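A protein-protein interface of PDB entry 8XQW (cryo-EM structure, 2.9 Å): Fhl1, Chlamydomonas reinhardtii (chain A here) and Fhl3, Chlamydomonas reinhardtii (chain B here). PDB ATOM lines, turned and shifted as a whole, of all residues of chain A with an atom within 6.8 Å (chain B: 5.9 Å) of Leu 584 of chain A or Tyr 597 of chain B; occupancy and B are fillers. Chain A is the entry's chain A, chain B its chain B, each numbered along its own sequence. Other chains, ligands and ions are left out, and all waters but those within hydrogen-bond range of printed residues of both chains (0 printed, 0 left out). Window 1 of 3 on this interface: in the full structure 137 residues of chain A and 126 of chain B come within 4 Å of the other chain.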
ATOM      1  N   VAL A 540       1.747 -24.338  -9.531  1.00  0.00           N
ATOM      2  CA  VAL A 540       1.587 -23.793 -10.880  1.00  0.00           C
ATOM      3  C   VAL A 540       1.320 -24.918 -11.869  1.00  0.00           C
ATOM      4  O   VAL A 540       0.588 -24.745 -12.850  1.00  0.00           O
ATOM      5  CB  VAL A 540       2.809 -22.951 -11.289  1.00  0.00           C
ATOM      6  CG1 VAL A 540       2.786 -21.625 -10.571  1.00  0.00           C
ATOM      7  CG2 VAL A 540       4.089 -23.678 -11.000  1.00  0.00           C
ATOM      8  N   ARG A 567      15.765 -13.759 -12.509  1.00  0.00           N
ATOM      9  CA  ARG A 567      16.656 -14.554 -11.671  1.00  0.00           C
ATOM     10  C   ARG A 567      17.971 -13.802 -11.531  1.00  0.00           C
ATOM     11  O   ARG A 567      18.551 -13.349 -12.521  1.00  0.00           O
ATOM     12  CB  ARG A 567      16.883 -15.933 -12.272  1.00  0.00           C
ATOM     13  CG  ARG A 567      15.694 -16.501 -12.999  1.00  0.00           C
ATOM     14  CD  ARG A 567      16.080 -17.794 -13.672  1.00  0.00           C
ATOM     15  NE  ARG A 567      15.112 -18.200 -14.681  1.00  0.00           N
ATOM     16  CZ  ARG A 567      15.268 -19.257 -15.468  1.00  0.00           C
ATOM     17  NH1 ARG A 567      16.352 -20.008 -15.352  1.00  0.00           N
ATOM     18  NH2 ARG A 567      14.343 -19.565 -16.365  1.00  0.00           N
ATOM     19  N   MET A 577      15.547 -20.400  -4.442  1.00  0.00           N
ATOM     20  CA  MET A 577      15.369 -21.725  -5.017  1.00  0.00           C
ATOM     21  C   MET A 577      13.924 -21.961  -5.412  1.00  0.00           C
ATOM     22  O   MET A 577      13.637 -22.255  -6.580  1.00  0.00           O
ATOM     23  CB  MET A 577      15.809 -22.795  -4.020  1.00  0.00           C
ATOM     24  CG  MET A 577      17.153 -22.531  -3.385  1.00  0.00           C
ATOM     25  SD  MET A 577      18.390 -22.115  -4.614  1.00  0.00           S
ATOM     26  CE  MET A 577      18.875 -23.762  -5.112  1.00  0.00           C
ATOM     27  N   ARG A 579      11.461 -19.819  -5.706  1.00  0.00           N
ATOM     28  CA  ARG A 579      10.933 -18.832  -6.640  1.00  0.00           C
ATOM     29  C   ARG A 579      11.338 -19.147  -8.072  1.00  0.00           C
ATOM     30  O   ARG A 579      10.488 -19.166  -8.970  1.00  0.00           O
ATOM     31  CB  ARG A 579      11.389 -17.431  -6.237  1.00  0.00           C
ATOM     32  CG  ARG A 579      10.333 -16.653  -5.472  1.00  0.00           C
ATOM     33  CD  ARG A 579      10.971 -15.617  -4.580  1.00  0.00           C
ATOM     34  NE  ARG A 579      11.350 -16.172  -3.286  1.00  0.00           N
ATOM     35  CZ  ARG A 579      10.765 -15.848  -2.139  1.00  0.00           C
ATOM     36  NH1 ARG A 579       9.779 -14.963  -2.126  1.00  0.00           N
ATOM     37  NH2 ARG A 579      11.170 -16.399  -1.006  1.00  0.00           N
ATOM     38  N   GLU A 580      12.619 -19.431  -8.317  1.00  0.00           N
ATOM     39  CA  GLU A 580      12.990 -19.693  -9.703  1.00  0.00           C
ATOM     40  C   GLU A 580      12.529 -21.076 -10.142  1.00  0.00           C
ATOM     41  O   GLU A 580      12.352 -21.310 -11.337  1.00  0.00           O
ATOM     42  CB  GLU A 580      14.494 -19.522  -9.942  1.00  0.00           C
ATOM     43  CG  GLU A 580      15.440 -20.175  -8.964  1.00  0.00           C
ATOM     44  CD  GLU A 580      15.472 -21.687  -9.062  1.00  0.00           C
ATOM     45  OE1 GLU A 580      15.898 -22.332  -8.082  1.00  0.00           O
ATOM     46  OE2 GLU A 580      15.096 -22.239 -10.116  1.00  0.00           O
ATOM     47  N   SER A 581      12.319 -22.005  -9.203  1.00  0.00           N
ATOM     48  CA  SER A 581      11.743 -23.291  -9.587  1.00  0.00           C
ATOM     49  C   SER A 581      10.307 -23.124 -10.063  1.00  0.00           C
ATOM     50  O   SER A 581       9.906 -23.691 -11.091  1.00  0.00           O
ATOM     51  CB  SER A 581      11.802 -24.266  -8.416  1.00  0.00           C
ATOM     52  OG  SER A 581      10.976 -23.821  -7.357  1.00  0.00           O
ATOM     53  N   ALA A 582       9.516 -22.347  -9.322  1.00  0.00           N
ATOM     54  CA  ALA A 582       8.191 -21.980  -9.798  1.00  0.00           C
ATOM     55  C   ALA A 582       8.276 -21.252 -11.128  1.00  0.00           C
ATOM     56  O   ALA A 582       7.405 -21.412 -11.988  1.00  0.00           O
ATOM     57  CB  ALA A 582       7.481 -21.118  -8.757  1.00  0.00           C
ATOM     58  N   LEU A 583       9.320 -20.446 -11.319  1.00  0.00           N
ATOM     59  CA  LEU A 583       9.485 -19.733 -12.580  1.00  0.00           C
ATOM     60  C   LEU A 583       9.723 -20.708 -13.726  1.00  0.00           C
ATOM     61  O   LEU A 583       9.139 -20.572 -14.806  1.00  0.00           O
ATOM     62  CB  LEU A 583      10.635 -18.734 -12.459  1.00  0.00           C
ATOM     63  CG  LEU A 583      10.675 -17.466 -13.314  1.00  0.00           C
ATOM     64  CD1 LEU A 583      11.946 -16.706 -13.009  1.00  0.00           C
ATOM     65  CD2 LEU A 583      10.584 -17.741 -14.796  1.00  0.00           C
ATOM     66  N   LEU A 584      10.600 -21.690 -13.511  1.00  0.00           N
ATOM     67  CA  LEU A 584      10.837 -22.720 -14.516  1.00  0.00           C
ATOM     68  C   LEU A 584       9.552 -23.447 -14.865  1.00  0.00           C
ATOM     69  O   LEU A 584       9.276 -23.702 -16.042  1.00  0.00           O
ATOM     70  CB  LEU A 584      11.870 -23.730 -14.024  1.00  0.00           C
ATOM     71  CG  LEU A 584      13.232 -23.278 -13.513  1.00  0.00           C
ATOM     72  CD1 LEU A 584      14.200 -24.439 -13.581  1.00  0.00           C
ATOM     73  CD2 LEU A 584      13.743 -22.111 -14.321  1.00  0.00           C
ATOM     74  N   ALA A 585       8.772 -23.816 -13.850  1.00  0.00           N
ATOM     75  CA  ALA A 585       7.527 -24.530 -14.112  1.00  0.00           C
ATOM     76  C   ALA A 585       6.565 -23.665 -14.911  1.00  0.00           C
ATOM     77  O   ALA A 585       5.995 -24.110 -15.911  1.00  0.00           O
ATOM     78  CB  ALA A 585       6.897 -24.982 -12.799  1.00  0.00           C
ATOM     79  N   MET A 586       6.361 -22.427 -14.460  1.00  0.00           N
ATOM     80  CA  MET A 586       5.599 -21.428 -15.200  1.00  0.00           C
ATOM     81  C   MET A 586       6.012 -21.377 -16.664  1.00  0.00           C
ATOM     82  O   MET A 586       5.158 -21.447 -17.560  1.00  0.00           O
ATOM     83  CB  MET A 586       5.818 -20.069 -14.533  1.00  0.00           C
ATOM     84  CG  MET A 586       4.662 -19.565 -13.687  1.00  0.00           C
ATOM     85  SD  MET A 586       3.133 -19.365 -14.598  1.00  0.00           S
ATOM     86  CE  MET A 586       3.747 -18.409 -15.975  1.00  0.00           C
ATOM     87  N   LEU A 587       7.317 -21.278 -16.916  1.00  0.00           N
ATOM     88  CA  LEU A 587       7.822 -21.232 -18.280  1.00  0.00           C
ATOM     89  C   LEU A 587       7.412 -22.476 -19.053  1.00  0.00           C
ATOM     90  O   LEU A 587       6.584 -22.404 -19.969  1.00  0.00           O
ATOM     91  CB  LEU A 587       9.343 -21.094 -18.262  1.00  0.00           C
ATOM     92  CG  LEU A 587       9.891 -19.675 -18.354  1.00  0.00           C
ATOM     93  CD1 LEU A 587      11.364 -19.645 -17.992  1.00  0.00           C
ATOM     94  CD2 LEU A 587       9.669 -19.127 -19.746  1.00  0.00           C
ATOM     95  N   VAL A 588       7.930 -23.637 -18.641  1.00  0.00           N
ATOM     96  CA  VAL A 588       7.743 -24.865 -19.409  1.00  0.00           C
ATOM     97  C   VAL A 588       6.263 -25.155 -19.621  1.00  0.00           C
ATOM     98  O   VAL A 588       5.878 -25.755 -20.632  1.00  0.00           O
ATOM     99  CB  VAL A 588       8.460 -26.039 -18.721  1.00  0.00           C
ATOM    100  CG1 VAL A 588       7.974 -26.198 -17.304  1.00  0.00           C
ATOM    101  CG2 VAL A 588       8.260 -27.320 -19.499  1.00  0.00           C
ATOM    102  N   GLN A 589       5.405 -24.706 -18.704  1.00  0.00           N
ATOM    103  CA  GLN A 589       3.974 -24.894 -18.894  1.00  0.00           C
ATOM    104  C   GLN A 589       3.441 -23.956 -19.963  1.00  0.00           C
ATOM    105  O   GLN A 589       2.693 -24.376 -20.851  1.00  0.00           O
ATOM    106  CB  GLN A 589       3.239 -24.677 -17.575  1.00  0.00           C
ATOM    107  CG  GLN A 589       3.470 -25.771 -16.567  1.00  0.00           C
ATOM    108  CD  GLN A 589       3.258 -27.142 -17.149  1.00  0.00           C
ATOM    109  OE1 GLN A 589       2.191 -27.444 -17.679  1.00  0.00           O
ATOM    110  NE2 GLN A 589       4.276 -27.989 -17.054  1.00  0.00           N
ATOM    111  N   MET A 590       3.808 -22.673 -19.898  1.00  0.00           N
ATOM    112  CA  MET A 590       3.200 -21.734 -20.832  1.00  0.00           C
ATOM    113  C   MET A 590       3.704 -21.949 -22.251  1.00  0.00           C
ATOM    114  O   MET A 590       2.927 -21.837 -23.203  1.00  0.00           O
ATOM    115  CB  MET A 590       3.449 -20.296 -20.395  1.00  0.00           C
ATOM    116  CG  MET A 590       2.740 -19.294 -21.285  1.00  0.00           C
ATOM    117  SD  MET A 590       3.091 -17.580 -20.890  1.00  0.00           S
ATOM    118  CE  MET A 590       3.919 -17.762 -19.326  1.00  0.00           C
ATOM    119  N   ASP A 591       4.990 -22.262 -22.415  1.00  0.00           N
ATOM    120  CA  ASP A 591       5.445 -22.742 -23.711  1.00  0.00           C
ATOM    121  C   ASP A 591       5.002 -24.172 -23.952  1.00  0.00           C
ATOM    122  O   ASP A 591       5.168 -24.690 -25.062  1.00  0.00           O
ATOM    123  CB  ASP A 591       6.963 -22.639 -23.833  1.00  0.00           C
ATOM    124  CG  ASP A 591       7.684 -23.332 -22.699  1.00  0.00           C
ATOM    125  OD1 ASP A 591       7.633 -24.575 -22.630  1.00  0.00           O
ATOM    126  OD2 ASP A 591       8.332 -22.633 -21.894  1.00  0.00           O
ATOM    127  N   GLY B 593      17.064 -26.086 -22.306  1.00  0.00           N
ATOM    128  CA  GLY B 593      17.825 -26.014 -21.045  1.00  0.00           C
ATOM    129  C   GLY B 593      16.962 -26.333 -19.850  1.00  0.00           C
ATOM    130  O   GLY B 593      17.425 -27.090 -18.976  1.00  0.00           O
ATOM    131  N   THR B 594      15.743 -25.797 -19.816  1.00  0.00           N
ATOM    132  CA  THR B 594      14.836 -25.983 -18.660  1.00  0.00           C
ATOM    133  C   THR B 594      14.754 -27.432 -18.251  1.00  0.00           C
ATOM    134  O   THR B 594      14.826 -27.696 -17.046  1.00  0.00           O
ATOM    135  CB  THR B 594      13.462 -25.457 -19.064  1.00  0.00           C
ATOM    136  OG1 THR B 594      13.180 -26.087 -20.309  1.00  0.00           O
ATOM    137  CG2 THR B 594      13.442 -23.948 -19.228  1.00  0.00           C
ATOM    138  N   ASP B 595      14.587 -28.337 -19.209  1.00  0.00           N
ATOM    139  CA  ASP B 595      14.397 -29.775 -18.898  1.00  0.00           C
ATOM    140  C   ASP B 595      15.440 -30.259 -17.899  1.00  0.00           C
ATOM    141  O   ASP B 595      15.094 -30.448 -16.727  1.00  0.00           O
ATOM    142  CB  ASP B 595      14.451 -30.584 -20.177  1.00  0.00           C
ATOM    143  CG  ASP B 595      13.858 -29.880 -21.389  1.00  0.00           C
ATOM    144  OD1 ASP B 595      13.138 -28.880 -21.193  1.00  0.00           O
ATOM    145  OD2 ASP B 595      14.124 -30.326 -22.521  1.00  0.00           O
ATOM    146  N   PHE B 596      16.662 -30.488 -18.362  1.00  0.00           N
ATOM    147  CA  PHE B 596      17.697 -31.064 -17.467  1.00  0.00           C
ATOM    148  C   PHE B 596      17.721 -30.306 -16.148  1.00  0.00           C
ATOM    149  O   PHE B 596      18.186 -30.893 -15.157  1.00  0.00           O
ATOM    150  CB  PHE B 596      19.074 -31.026 -18.127  1.00  0.00           C
ATOM    151  CG  PHE B 596      19.165 -31.616 -19.526  1.00  0.00           C
ATOM    152  CD1 PHE B 596      19.023 -30.812 -20.647  1.00  0.00           C
ATOM    153  CD2 PHE B 596      19.413 -32.969 -19.711  1.00  0.00           C
ATOM    154  CE1 PHE B 596      19.128 -31.349 -21.916  1.00  0.00           C
ATOM    155  CE2 PHE B 596      19.510 -33.502 -20.985  1.00  0.00           C
ATOM    156  CZ  PHE B 596      19.365 -32.691 -22.084  1.00  0.00           C
ATOM    157  N   TYR B 597      17.271 -29.050 -16.123  1.00  0.00           N
ATOM    158  CA  TYR B 597      17.364 -28.294 -14.885  1.00  0.00           C
ATOM    159  C   TYR B 597      16.193 -28.648 -13.979  1.00  0.00           C
ATOM    160  O   TYR B 597      15.030 -28.504 -14.369  1.00  0.00           O
ATOM    161  CB  TYR B 597      17.398 -26.791 -15.146  1.00  0.00           C
ATOM    162  CG  TYR B 597      18.061 -26.037 -14.020  1.00  0.00           C
ATOM    163  CD1 TYR B 597      19.004 -26.658 -13.213  1.00  0.00           C
ATOM    164  CD2 TYR B 597      17.740 -24.716 -13.751  1.00  0.00           C
ATOM    165  CE1 TYR B 597      19.613 -25.984 -12.179  1.00  0.00           C
ATOM    166  CE2 TYR B 597      18.344 -24.033 -12.715  1.00  0.00           C
ATOM    167  CZ  TYR B 597      19.281 -24.673 -11.932  1.00  0.00           C
ATOM    168  OH  TYR B 597      19.890 -24.003 -10.897  1.00  0.00           O
ATOM    169  N   ASP B 598      16.511 -29.109 -12.773  1.00  0.00           N
ATOM    170  CA  ASP B 598      15.509 -29.455 -11.776  1.00  0.00           C
ATOM    171  C   ASP B 598      16.210 -29.585 -10.435  1.00  0.00           C
ATOM    172  O   ASP B 598      17.205 -30.306 -10.321  1.00  0.00           O
ATOM    173  CB  ASP B 598      14.778 -30.741 -12.162  1.00  0.00           C
ATOM    174  CG  ASP B 598      15.719 -31.837 -12.609  1.00  0.00           C
ATOM    175  OD1 ASP B 598      16.941 -31.594 -12.662  1.00  0.00           O
ATOM    176  OD2 ASP B 598      15.233 -32.945 -12.925  1.00  0.00           O
ATOM    177  N   VAL B 599      15.695 -28.881  -9.425  1.00  0.00           N
ATOM    178  CA  VAL B 599      16.438 -28.690  -8.184  1.00  0.00           C
ATOM    179  C   VAL B 599      16.590 -29.974  -7.383  1.00  0.00           C
ATOM    180  O   VAL B 599      17.516 -30.087  -6.572  1.00  0.00           O
ATOM    181  CB  VAL B 599      15.764 -27.591  -7.339  1.00  0.00           C
ATOM    182  CG1 VAL B 599      15.869 -26.247  -8.048  1.00  0.00           C
ATOM    183  CG2 VAL B 599      14.312 -27.949  -7.060  1.00  0.00           C
ATOM    184  N   ALA B 630      20.619 -21.876 -19.615  1.00  0.00           N
ATOM    185  CA  ALA B 630      19.917 -22.421 -18.459  1.00  0.00           C
ATOM    186  C   ALA B 630      20.733 -23.519 -17.797  1.00  0.00           C
ATOM    187  O   ALA B 630      20.772 -23.617 -16.565  1.00  0.00           O
ATOM    188  CB  ALA B 630      18.541 -22.941 -18.874  1.00  0.00           C
ATOM    189  N   MET B 631      21.395 -24.355 -18.595  1.00  0.00           N
ATOM    190  CA  MET B 631      22.357 -25.302 -18.050  1.00  0.00           C
ATOM    191  C   MET B 631      23.770 -24.739 -18.091  1.00  0.00           C
ATOM    192  O   MET B 631      24.564 -24.962 -17.173  1.00  0.00           O
ATOM    193  CB  MET B 631      22.307 -26.623 -18.818  1.00  0.00           C
ATOM    194  CG  MET B 631      20.923 -27.174 -19.030  1.00  0.00           C
ATOM    195  SD  MET B 631      20.771 -27.824 -20.696  1.00  0.00           S
ATOM    196  CE  MET B 631      22.261 -28.811 -20.794  1.00  0.00           C
ATOM    197  N   ALA B 637      26.779 -20.592  -9.421  1.00  0.00           N
ATOM    198  CA  ALA B 637      25.361 -20.539  -9.711  1.00  0.00           C
ATOM    199  C   ALA B 637      24.597 -21.084  -8.509  1.00  0.00           C
ATOM    200  O   ALA B 637      25.178 -21.397  -7.465  1.00  0.00           O
ATOM    201  CB  ALA B 637      25.053 -21.315 -10.995  1.00  0.00           C
ATOM    202  N   GLN B 638      23.283 -21.204  -8.646  1.00  0.00           N
ATOM    203  CA  GLN B 638      22.463 -21.656  -7.527  1.00  0.00           C
ATOM    204  C   GLN B 638      22.658 -23.154  -7.354  1.00  0.00           C
ATOM    205  O   GLN B 638      21.904 -23.967  -7.892  1.00  0.00           O
ATOM    206  CB  GLN B 638      20.998 -21.297  -7.745  1.00  0.00           C
ATOM    207  CG  GLN B 638      20.664 -19.860  -7.358  1.00  0.00           C
ATOM    208  CD  GLN B 638      21.503 -19.342  -6.193  1.00  0.00           C
ATOM    209  OE1 GLN B 638      22.293 -18.411  -6.351  1.00  0.00           O
ATOM    210  NE2 GLN B 638      21.323 -19.937  -5.018  1.00  0.00           N
ATOM    211  N   ALA B 639      23.689 -23.513  -6.601  1.00  0.00           N
ATOM    212  CA  ALA B 639      23.981 -24.891  -6.225  1.00  0.00           C
ATOM    213  C   ALA B 639      24.970 -24.837  -5.070  1.00  0.00           C
ATOM    214  O   ALA B 639      25.394 -23.761  -4.640  1.00  0.00           O
ATOM    215  CB  ALA B 639      24.534 -25.694  -7.403  1.00  0.00           C
ATOM    216  N   GLU B 643      23.984 -30.141  -8.026  1.00  0.00           N
ATOM    217  CA  GLU B 643      23.149 -30.398  -9.197  1.00  0.00           C
ATOM    218  C   GLU B 643      23.725 -29.798 -10.476  1.00  0.00           C
ATOM    219  O   GLU B 643      24.062 -30.529 -11.411  1.00  0.00           O
ATOM    220  CB  GLU B 643      21.732 -29.867  -8.959  1.00  0.00           C
ATOM    221  CG  GLU B 643      20.739 -30.296 -10.024  1.00  0.00           C
ATOM    222  CD  GLU B 643      20.437 -31.780  -9.968  1.00  0.00           C
ATOM    223  OE1 GLU B 643      20.229 -32.390 -11.036  1.00  0.00           O
ATOM    224  OE2 GLU B 643      20.407 -32.338  -8.855  1.00  0.00           O
ATOM    225  N   SER B 644      23.853 -28.471 -10.533  1.00  0.00           N
ATOM    226  CA  SER B 644      24.338 -27.848 -11.760  1.00  0.00           C
ATOM    227  C   SER B 644      25.796 -28.205 -12.006  1.00  0.00           C
ATOM    228  O   SER B 644      26.223 -28.372 -13.155  1.00  0.00           O
ATOM    229  CB  SER B 644      24.160 -26.336 -11.692  1.00  0.00           C
ATOM    230  OG  SER B 644      24.956 -25.793 -10.659  1.00  0.00           O
ATOM    231  N   ILE B 647      25.724 -31.592 -13.719  1.00  0.00           N
ATOM    232  CA  ILE B 647      25.288 -31.610 -15.112  1.00  0.00           C
ATOM    233  C   ILE B 647      26.345 -30.982 -16.008  1.00  0.00           C
ATOM    234  O   ILE B 647      26.545 -31.413 -17.150  1.00  0.00           O
ATOM    235  CB  ILE B 647      23.921 -30.921 -15.269  1.00  0.00           C
ATOM    236  CG1 ILE B 647      24.039 -29.414 -15.096  1.00  0.00           C
ATOM    237  CG2 ILE B 647      22.943 -31.472 -14.256  1.00  0.00           C
ATOM    238  CD1 ILE B 647      23.135 -28.644 -16.005  1.00  0.00           C
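Printed residues of chain B that touch a printed residue of chain A: Tyr 597, Val 599 and Gln 638.
Along chain B the printed residues that touch a printed residue of chain A span positions 597 to 638.
OE1 of Glu 580 of chain A sits close to O of Met 577 of chain A.
The side-chain hydroxyl (OG) of Ser 581 of chain A lies within hydrogen-bond range of the backbone carbonyl oxygen (O) of Met 577 of chain A (3.2 Å).
NE2 of Gln 638 of chain B lies within hydrogen-bond range of SD of Met 577 of chain A (3.7 Å).
Printed residues of chain B within 4 Å of Met 577 of chain A: Gln 638.
Leu 584 of chain A touches just one residue of chain B: Tyr 597 (3.6 Å).
Gln 589 of chain A touches none of the printed residues of chain B.
Of chain A, only Leu 584 comes within 4 Å of Tyr 597 of chain B.
Printed residues of chain A within 4 Å of Val 599 of chain B: Glu 580 (3.9 Å).
The nearest printed residue of chain B that does not touch Met 577 of chain A is Val 599 of chain B (4.8 Å).
Val 599 of chain B touches Glu 580 of chain A.
Tyr 597 of chain B touches Leu 584 of chain A.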
